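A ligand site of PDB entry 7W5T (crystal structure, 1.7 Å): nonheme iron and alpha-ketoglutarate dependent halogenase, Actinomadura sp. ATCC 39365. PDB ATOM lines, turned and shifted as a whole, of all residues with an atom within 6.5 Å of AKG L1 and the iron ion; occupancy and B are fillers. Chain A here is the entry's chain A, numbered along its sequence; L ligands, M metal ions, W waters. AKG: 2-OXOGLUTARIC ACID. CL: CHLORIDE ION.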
ATOM      1  N   LYS A 117       6.870   5.971  25.329  1.00  0.00           N
ATOM      2  CA  LYS A 117       7.612   4.731  24.955  1.00  0.00           C
ATOM      3  C   LYS A 117       7.826   4.713  23.448  1.00  0.00           C
ATOM      4  O   LYS A 117       7.013   5.332  22.666  1.00  0.00           O
ATOM      5  CB  LYS A 117       6.776   3.516  25.416  1.00  0.00           C
ATOM      6  CG  LYS A 117       5.438   3.347  24.698  1.00  0.00           C
ATOM      7  CD  LYS A 117       4.542   2.283  25.164  1.00  0.00           C
ATOM      8  CE  LYS A 117       3.305   2.179  24.297  1.00  0.00           C
ATOM      9  NZ  LYS A 117       2.286   1.339  24.942  1.00  0.00           N
ATOM     10  N   ARG A 187       6.300  -7.969  21.193  1.00  0.00           N
ATOM     11  CA  ARG A 187       6.442  -6.529  21.395  1.00  0.00           C
ATOM     12  C   ARG A 187       7.582  -6.311  22.391  1.00  0.00           C
ATOM     13  O   ARG A 187       7.589  -6.945  23.465  1.00  0.00           O
ATOM     14  CB  ARG A 187       5.153  -5.955  21.962  1.00  0.00           C
ATOM     15  CG  ARG A 187       5.287  -4.492  22.304  1.00  0.00           C
ATOM     16  CD  ARG A 187       4.021  -3.911  22.906  1.00  0.00           C
ATOM     17  NE  ARG A 187       3.101  -3.533  21.886  1.00  0.00           N
ATOM     18  CZ  ARG A 187       2.013  -2.797  22.083  1.00  0.00           C
ATOM     19  NH1 ARG A 187       1.656  -2.408  23.300  1.00  0.00           N
ATOM     20  NH2 ARG A 187       1.285  -2.440  21.017  1.00  0.00           N
ATOM     21  N   ILE A 189       9.496  -3.142  24.372  1.00  0.00           N
ATOM     22  CA  ILE A 189       9.098  -1.757  24.721  1.00  0.00           C
ATOM     23  C   ILE A 189      10.243  -1.093  25.487  1.00  0.00           C
ATOM     24  O   ILE A 189      10.747  -1.674  26.477  1.00  0.00           O
ATOM     25  CB  ILE A 189       7.828  -1.718  25.580  1.00  0.00           C
ATOM     26  CG1 ILE A 189       6.701  -2.597  25.039  1.00  0.00           C
ATOM     27  CG2 ILE A 189       7.377  -0.271  25.815  1.00  0.00           C
ATOM     28  CD1 ILE A 189       5.725  -3.057  26.110  1.00  0.00           C
ATOM     29  N   TYR A 191      10.393   2.352  27.529  1.00  0.00           N
ATOM     30  CA  TYR A 191       9.804   3.530  28.156  1.00  0.00           C
ATOM     31  C   TYR A 191      10.956   4.488  28.485  1.00  0.00           C
ATOM     32  O   TYR A 191      12.008   4.098  29.066  1.00  0.00           O
ATOM     33  CB  TYR A 191       9.046   3.162  29.426  1.00  0.00           C
ATOM     34  CG  TYR A 191       7.898   2.184  29.304  1.00  0.00           C
ATOM     35  CD1 TYR A 191       8.099   0.815  29.341  1.00  0.00           C
ATOM     36  CD2 TYR A 191       6.612   2.654  29.106  1.00  0.00           C
ATOM     37  CE1 TYR A 191       7.016  -0.068  29.211  1.00  0.00           C
ATOM     38  CE2 TYR A 191       5.542   1.796  29.005  1.00  0.00           C
ATOM     39  CZ  TYR A 191       5.736   0.432  29.071  1.00  0.00           C
ATOM     40  OH  TYR A 191       4.628  -0.371  28.960  1.00  0.00           O
ATOM     41  N   ALA A 201       1.221   2.650  31.306  1.00  0.00           N
ATOM     42  CA  ALA A 201       0.258   1.928  30.429  1.00  0.00           C
ATOM     43  C   ALA A 201      -1.103   1.921  31.125  1.00  0.00           C
ATOM     44  O   ALA A 201      -1.180   1.430  32.220  1.00  0.00           O
ATOM     45  CB  ALA A 201       0.712   0.529  30.114  1.00  0.00           C
ATOM     46  N   HIS A 204      -5.945  -2.014  30.473  1.00  0.00           N
ATOM     47  CA  HIS A 204      -6.280  -2.580  29.158  1.00  0.00           C
ATOM     48  C   HIS A 204      -6.148  -4.095  29.156  1.00  0.00           C
ATOM     49  O   HIS A 204      -5.586  -4.641  30.101  1.00  0.00           O
ATOM     50  CB  HIS A 204      -5.349  -2.030  28.083  1.00  0.00           C
ATOM     51  CG  HIS A 204      -3.938  -2.494  28.120  1.00  0.00           C
ATOM     52  ND1 HIS A 204      -3.043  -2.010  29.059  1.00  0.00           N
ATOM     53  CD2 HIS A 204      -3.313  -3.541  27.497  1.00  0.00           C
ATOM     54  CE1 HIS A 204      -1.925  -2.642  28.917  1.00  0.00           C
ATOM     55  NE2 HIS A 204      -2.062  -3.593  27.978  1.00  0.00           N
ATOM     56  N   SER A 205      -6.581  -4.712  28.070  1.00  0.00           N
ATOM     57  CA  SER A 205      -6.277  -6.128  27.771  1.00  0.00           C
ATOM     58  C   SER A 205      -5.936  -6.264  26.313  1.00  0.00           C
ATOM     59  O   SER A 205      -6.137  -5.306  25.542  1.00  0.00           O
ATOM     60  CB  SER A 205      -7.434  -6.996  28.109  1.00  0.00           C
ATOM     61  OG  SER A 205      -8.533  -6.679  27.272  1.00  0.00           O
ATOM     62  N   GLY A 206      -5.315  -7.364  25.960  1.00  0.00           N
ATOM     63  CA  GLY A 206      -4.946  -7.634  24.567  1.00  0.00           C
ATOM     64  C   GLY A 206      -6.167  -8.024  23.768  1.00  0.00           C
ATOM     65  O   GLY A 206      -7.063  -8.733  24.290  1.00  0.00           O
ATOM     66  N   GLN A 213       3.684 -12.342  29.060  1.00  0.00           N
ATOM     67  CA  GLN A 213       4.442 -11.231  29.624  1.00  0.00           C
ATOM     68  C   GLN A 213       5.760 -11.825  30.124  1.00  0.00           C
ATOM     69  O   GLN A 213       5.749 -12.697  30.995  1.00  0.00           O
ATOM     70  CB  GLN A 213       3.649 -10.552  30.709  1.00  0.00           C
ATOM     71  CG  GLN A 213       4.458  -9.511  31.433  1.00  0.00           C
ATOM     72  CD  GLN A 213       4.775  -8.343  30.553  1.00  0.00           C
ATOM     73  OE1 GLN A 213       3.844  -7.767  29.995  1.00  0.00           O
ATOM     74  NE2 GLN A 213       6.056  -7.992  30.485  1.00  0.00           N
ATOM     75  N   LEU A 214       6.852 -11.343  29.591  1.00  0.00           N
ATOM     76  CA  LEU A 214       8.197 -11.814  29.957  1.00  0.00           C
ATOM     77  C   LEU A 214       8.714 -10.920  31.074  1.00  0.00           C
ATOM     78  O   LEU A 214       8.224  -9.811  31.277  1.00  0.00           O
ATOM     79  CB  LEU A 214       9.048 -11.744  28.713  1.00  0.00           C
ATOM     80  CG  LEU A 214       8.543 -12.620  27.550  1.00  0.00           C
ATOM     81  CD1 LEU A 214       9.290 -12.271  26.325  1.00  0.00           C
ATOM     82  CD2 LEU A 214       8.734 -14.102  27.838  1.00  0.00           C
ATOM     83  N   PRO A 216      10.088  -8.120  33.078  1.00  0.00           N
ATOM     84  CA  PRO A 216      10.525  -6.780  32.689  1.00  0.00           C
ATOM     85  C   PRO A 216      11.736  -6.305  33.513  1.00  0.00           C
ATOM     86  O   PRO A 216      12.138  -6.925  34.484  1.00  0.00           O
ATOM     87  CB  PRO A 216       9.322  -5.912  32.999  1.00  0.00           C
ATOM     88  CG  PRO A 216       8.584  -6.640  34.097  1.00  0.00           C
ATOM     89  CD  PRO A 216       8.946  -8.095  33.983  1.00  0.00           C
ATOM     90  N   ASP A 218      11.812  -3.643  35.447  1.00  0.00           N
ATOM     91  CA  ASP A 218      11.407  -2.951  36.684  1.00  0.00           C
ATOM     92  C   ASP A 218       9.981  -3.340  37.028  1.00  0.00           C
ATOM     93  O   ASP A 218       9.241  -3.844  36.169  1.00  0.00           O
ATOM     94  CB  ASP A 218      11.500  -1.437  36.570  1.00  0.00           C
ATOM     95  CG  ASP A 218      11.651  -0.722  37.913  1.00  0.00           C
ATOM     96  OD1 ASP A 218      11.552  -1.375  39.009  1.00  0.00           O
ATOM     97  OD2 ASP A 218      11.830   0.530  37.832  1.00  0.00           O
ATOM     98  N   GLY A 220       6.000  -2.435  38.378  1.00  0.00           N
ATOM     99  CA  GLY A 220       4.972  -1.484  37.929  1.00  0.00           C
ATOM    100  C   GLY A 220       3.820  -2.152  37.238  1.00  0.00           C
ATOM    101  O   GLY A 220       2.754  -1.573  37.217  1.00  0.00           O
ATOM    102  N   LEU A 221       4.035  -3.283  36.595  1.00  0.00           N
ATOM    103  CA  LEU A 221       2.912  -3.979  35.932  1.00  0.00           C
ATOM    104  C   LEU A 221       2.017  -4.533  37.035  1.00  0.00           C
ATOM    105  O   LEU A 221       2.526  -5.221  37.929  1.00  0.00           O
ATOM    106  CB  LEU A 221       3.465  -5.117  35.081  1.00  0.00           C
ATOM    107  CG  LEU A 221       2.435  -5.983  34.344  1.00  0.00           C
ATOM    108  CD1 LEU A 221       1.593  -5.197  33.371  1.00  0.00           C
ATOM    109  CD2 LEU A 221       3.146  -7.128  33.673  1.00  0.00           C
ATOM    110  N   ILE A 235       7.910  -9.545  39.479  1.00  0.00           N
ATOM    111  CA  ILE A 235       8.405 -10.194  38.226  1.00  0.00           C
ATOM    112  C   ILE A 235       9.693  -9.548  37.739  1.00  0.00           C
ATOM    113  O   ILE A 235      10.423 -10.219  36.994  1.00  0.00           O
ATOM    114  CB  ILE A 235       7.310 -10.240  37.143  1.00  0.00           C
ATOM    115  CG1 ILE A 235       6.794  -8.851  36.822  1.00  0.00           C
ATOM    116  CG2 ILE A 235       6.233 -11.240  37.528  1.00  0.00           C
ATOM    117  CD1 ILE A 235       5.841  -8.784  35.649  1.00  0.00           C
ATOM    118  N   ASN A 244      -1.682 -14.115  29.819  1.00  0.00           N
ATOM    119  CA  ASN A 244      -2.845 -13.226  29.841  1.00  0.00           C
ATOM    120  C   ASN A 244      -3.899 -13.805  28.921  1.00  0.00           C
ATOM    121  O   ASN A 244      -3.589 -14.114  27.747  1.00  0.00           O
ATOM    122  CB  ASN A 244      -2.490 -11.826  29.297  1.00  0.00           C
ATOM    123  CG  ASN A 244      -1.318 -11.137  29.971  1.00  0.00           C
ATOM    124  OD1 ASN A 244      -0.679 -10.246  29.356  1.00  0.00           O
ATOM    125  ND2 ASN A 244      -1.058 -11.452  31.205  1.00  0.00           N
ATOM    126  N   HIS A 262      -4.835  -5.413  32.785  1.00  0.00           N
ATOM    127  CA  HIS A 262      -3.564  -5.054  33.410  1.00  0.00           C
ATOM    128  C   HIS A 262      -3.248  -3.576  33.110  1.00  0.00           C
ATOM    129  O   HIS A 262      -3.936  -2.976  32.282  1.00  0.00           O
ATOM    130  CB  HIS A 262      -2.478  -6.054  33.055  1.00  0.00           C
ATOM    131  CG  HIS A 262      -2.263  -6.199  31.596  1.00  0.00           C
ATOM    132  ND1 HIS A 262      -2.998  -7.076  30.837  1.00  0.00           N
ATOM    133  CD2 HIS A 262      -1.389  -5.585  30.789  1.00  0.00           C
ATOM    134  CE1 HIS A 262      -2.622  -6.924  29.577  1.00  0.00           C
ATOM    135  NE2 HIS A 262      -1.629  -6.019  29.506  1.00  0.00           N
ATOM    136  N   ARG A 263      -2.200  -3.081  33.773  1.00  0.00           N
ATOM    137  CA  ARG A 263      -1.747  -1.676  33.646  1.00  0.00           C
ATOM    138  C   ARG A 263      -0.301  -1.570  34.114  1.00  0.00           C
ATOM    139  O   ARG A 263       0.217  -2.501  34.788  1.00  0.00           O
ATOM    140  CB  ARG A 263      -2.749  -0.855  34.458  1.00  0.00           C
ATOM    141  CG  ARG A 263      -2.522  -0.906  35.941  1.00  0.00           C
ATOM    142  CD  ARG A 263      -3.612  -0.253  36.748  1.00  0.00           C
ATOM    143  NE  ARG A 263      -3.253  -0.357  38.161  1.00  0.00           N
ATOM    144  CZ  ARG A 263      -4.086  -0.051  39.161  1.00  0.00           C
ATOM    145  NH1 ARG A 263      -5.296   0.409  38.853  1.00  0.00           N
ATOM    146  NH2 ARG A 263      -3.691  -0.155  40.430  1.00  0.00           N
ATOM    147  N   VAL A 264       0.348  -0.448  33.846  1.00  0.00           N
ATOM    148  CA  VAL A 264       1.711  -0.229  34.358  1.00  0.00           C
ATOM    149  C   VAL A 264       1.685   1.100  35.070  1.00  0.00           C
ATOM    150  O   VAL A 264       1.333   2.060  34.426  1.00  0.00           O
ATOM    151  CB  VAL A 264       2.770  -0.268  33.244  1.00  0.00           C
ATOM    152  CG1 VAL A 264       4.154  -0.050  33.820  1.00  0.00           C
ATOM    153  CG2 VAL A 264       2.672  -1.598  32.537  1.00  0.00           C
ATOM    154  N   ARG A 275      12.516   2.023  31.383  1.00  0.00           N
ATOM    155  CA  ARG A 275      11.963   0.685  31.703  1.00  0.00           C
ATOM    156  C   ARG A 275      11.914  -0.096  30.399  1.00  0.00           C
ATOM    157  O   ARG A 275      11.582   0.510  29.375  1.00  0.00           O
ATOM    158  CB  ARG A 275      10.571   0.765  32.361  1.00  0.00           C
ATOM    159  CG  ARG A 275       9.997  -0.575  32.825  1.00  0.00           C
ATOM    160  CD  ARG A 275       8.855  -0.419  33.826  1.00  0.00           C
ATOM    161  NE  ARG A 275       8.116  -1.680  34.101  1.00  0.00           N
ATOM    162  CZ  ARG A 275       7.334  -2.279  33.228  1.00  0.00           C
ATOM    163  NH1 ARG A 275       7.112  -1.665  32.078  1.00  0.00           N
ATOM    164  NH2 ARG A 275       6.669  -3.406  33.507  1.00  0.00           N
ATOM    165  N   LEU A 276      12.257  -1.376  30.463  1.00  0.00           N
ATOM    166  CA  LEU A 276      12.182  -2.272  29.300  1.00  0.00           C
ATOM    167  C   LEU A 276      11.233  -3.408  29.642  1.00  0.00           C
ATOM    168  O   LEU A 276      11.310  -3.926  30.777  1.00  0.00           O
ATOM    169  CB  LEU A 276      13.556  -2.827  28.999  1.00  0.00           C
ATOM    170  CG  LEU A 276      14.548  -1.819  28.376  1.00  0.00           C
ATOM    171  CD1 LEU A 276      15.981  -2.316  28.516  1.00  0.00           C
ATOM    172  CD2 LEU A 276      14.207  -1.634  26.919  1.00  0.00           C
ATOM    173  N   SER A 277      10.374  -3.733  28.701  1.00  0.00           N
ATOM    174  CA  SER A 277       9.406  -4.819  28.900  1.00  0.00           C
ATOM    175  C   SER A 277       9.130  -5.477  27.570  1.00  0.00           C
ATOM    176  O   SER A 277       9.128  -4.790  26.526  1.00  0.00           O
ATOM    177  CB  SER A 277       8.155  -4.300  29.512  1.00  0.00           C
ATOM    178  OG  SER A 277       7.370  -5.416  29.912  1.00  0.00           O
ATOM    179  N   SER A 278       8.833  -6.772  27.591  1.00  0.00           N
ATOM    180  CA  SER A 278       8.479  -7.456  26.335  1.00  0.00           C
ATOM    181  C   SER A 278       7.345  -8.411  26.630  1.00  0.00           C
ATOM    182  O   SER A 278       7.287  -9.016  27.768  1.00  0.00           O
ATOM    183  CB  SER A 278       9.669  -8.179  25.723  1.00  0.00           C
ATOM    184  OG  SER A 278      10.215  -9.027  26.665  1.00  0.00           O
ATOM    185  N   VAL A 279       6.500  -8.575  25.641  1.00  0.00           N
ATOM    186  CA  VAL A 279       5.277  -9.412  25.725  1.00  0.00           C
ATOM    187  C   VAL A 279       4.999 -10.010  24.368  1.00  0.00           C
ATOM    188  O   VAL A 279       5.170  -9.328  23.313  1.00  0.00           O
ATOM    189  CB  VAL A 279       4.081  -8.615  26.293  1.00  0.00           C
ATOM    190  CG1 VAL A 279       3.806  -7.369  25.536  1.00  0.00           C
ATOM    191  CG2 VAL A 279       2.826  -9.461  26.331  1.00  0.00           C
ATOM    192  N   PHE A 281       2.271 -11.404  21.869  1.00  0.00           N
ATOM    193  CA  PHE A 281       0.835 -11.370  21.549  1.00  0.00           C
ATOM    194  C   PHE A 281       0.529 -12.492  20.581  1.00  0.00           C
ATOM    195  O   PHE A 281       0.929 -12.401  19.378  1.00  0.00           O
ATOM    196  CB  PHE A 281       0.442 -10.009  20.944  1.00  0.00           C
ATOM    197  CG  PHE A 281       0.722  -8.812  21.839  1.00  0.00           C
ATOM    198  CD1 PHE A 281       0.399  -8.785  23.167  1.00  0.00           C
ATOM    199  CD2 PHE A 281       1.220  -7.648  21.277  1.00  0.00           C
ATOM    200  CE1 PHE A 281       0.629  -7.645  23.950  1.00  0.00           C
ATOM    201  CE2 PHE A 281       1.392  -6.503  22.037  1.00  0.00           C
ATOM    202  CZ  PHE A 281       1.073  -6.498  23.376  1.00  0.00           C
HETATM  203  C1  AKG L   1       1.483  -3.983  26.670  1.00  0.00           C
HETATM  204  O1  AKG L   1       0.409  -4.405  26.269  1.00  0.00           O
HETATM  205  O2  AKG L   1       2.251  -3.388  25.885  1.00  0.00           O
HETATM  206  C2  AKG L   1       1.752  -4.099  28.025  1.00  0.00           C
HETATM  207  O5  AKG L   1       0.863  -4.524  28.825  1.00  0.00           O
HETATM  208  C3  AKG L   1       3.038  -3.579  28.619  1.00  0.00           C
HETATM  209  C4  AKG L   1       3.470  -4.227  29.902  1.00  0.00           C
HETATM  210  C5  AKG L   1       4.777  -3.776  30.530  1.00  0.00           C
HETATM  211  O3  AKG L   1       5.290  -2.709  30.156  1.00  0.00           O
HETATM  212  O4  AKG L   1       5.217  -4.479  31.464  1.00  0.00           O
HETATM  213 CL    CL L   2      -2.107  -6.254  26.368  1.00  0.00          CL
HETATM  214 FE    FE M   1      -0.755  -5.320  27.754  1.00  0.00          FE
HETATM  215  O   HOH W   1       0.289  -7.092  27.534  1.00  0.00           O
HETATM  216  O   HOH W   2       2.919  -0.680  26.649  1.00  0.00           O
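Water W1 binds the iron ion (2.1 Å).
NE2 of His 262 binds the iron ion (2.1 Å).
The iron ion is bound by an oxygen (O5) of AKG L1 (2.1 Å).
O1 of AKG L1 is bound to the iron ion.
The iron ion is bound by CL of CL L2 (2.1 Å).
A ring nitrogen (NE2) of His 204 is bound to the iron ion, 2.2 Å away.
The iron ion has six donor atoms within binding distance.
N of Tyr 191 is in hydrogen-bond range of O of Arg 275, 2.9 Å away.
NE of Arg 275 lies within hydrogen-bond range of O of Asp 218, at 3.2 Å.
The backbone carbonyl oxygen (O) of Ser 277 sits at hydrogen-bond distance from the backbone NH (N) of Ile 189 (2.7 Å).
The side-chain amide nitrogen (NE2) of Gln 213 sits at hydrogen-bond distance from the side-chain hydroxyl (OG) of Ser 277 (2.9 Å).
N of Arg 187 lies within hydrogen-bond range of O of Val 279, 2.8 Å away.
NE2 of Gln 213 is in hydrogen-bond range of O of Ser 278.
The backbone NH (N) of Val 264 sits at hydrogen-bond distance from the backbone carbonyl oxygen (O) of Ala 201.
Ile 189 touches AKG L1 (CD1 to O2, 3.5 Å).
OE1 of Gln 213 touches C4 of AKG L1, at 3.6 Å.
Val 264 touches AKG L1.
Phe 281 touches AKG L1.
Hydrophobic or aromatic side chains within 4 Å of AKG L1: Ile 189, Tyr 191, His 204, His 262, Val 264 and Phe 281.
Within 4 Å of AKG L1: Arg 187, Ile 189, Tyr 191, His 204, Gln 213, His 262, Val 264, Arg 275, Ser 277 and Phe 281.
Along chain A the residues within 4 Å of AKG L1 span positions 187 to 281.
The nearest printed residue that does not touch AKG L1 is Leu 221 (4.02 Å).
The side-chain hydroxyl (OH) of Tyr 191 is in hydrogen-bond range of an oxygen (O3) of AKG L1 (2.7 Å).
The guanidinium group of Arg 275 is in salt-bridge range of an oxygen (O4) of AKG L1, at 2.7 Å.
OG of Ser 277 is in hydrogen-bond range of O4 of AKG L1 (2.8 Å).
The guanidinium group (NH1) of Arg 187 is in salt-bridge range of an oxygen (O2) of AKG L1.
Within 4 Å of the iron ion: His 204 and His 262.
Water W2 lies within hydrogen-bond range of NZ of Lys 117 (2.7 Å), OH of Tyr 191 (2.9 Å) and O2 of AKG L1 (2.9 Å).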
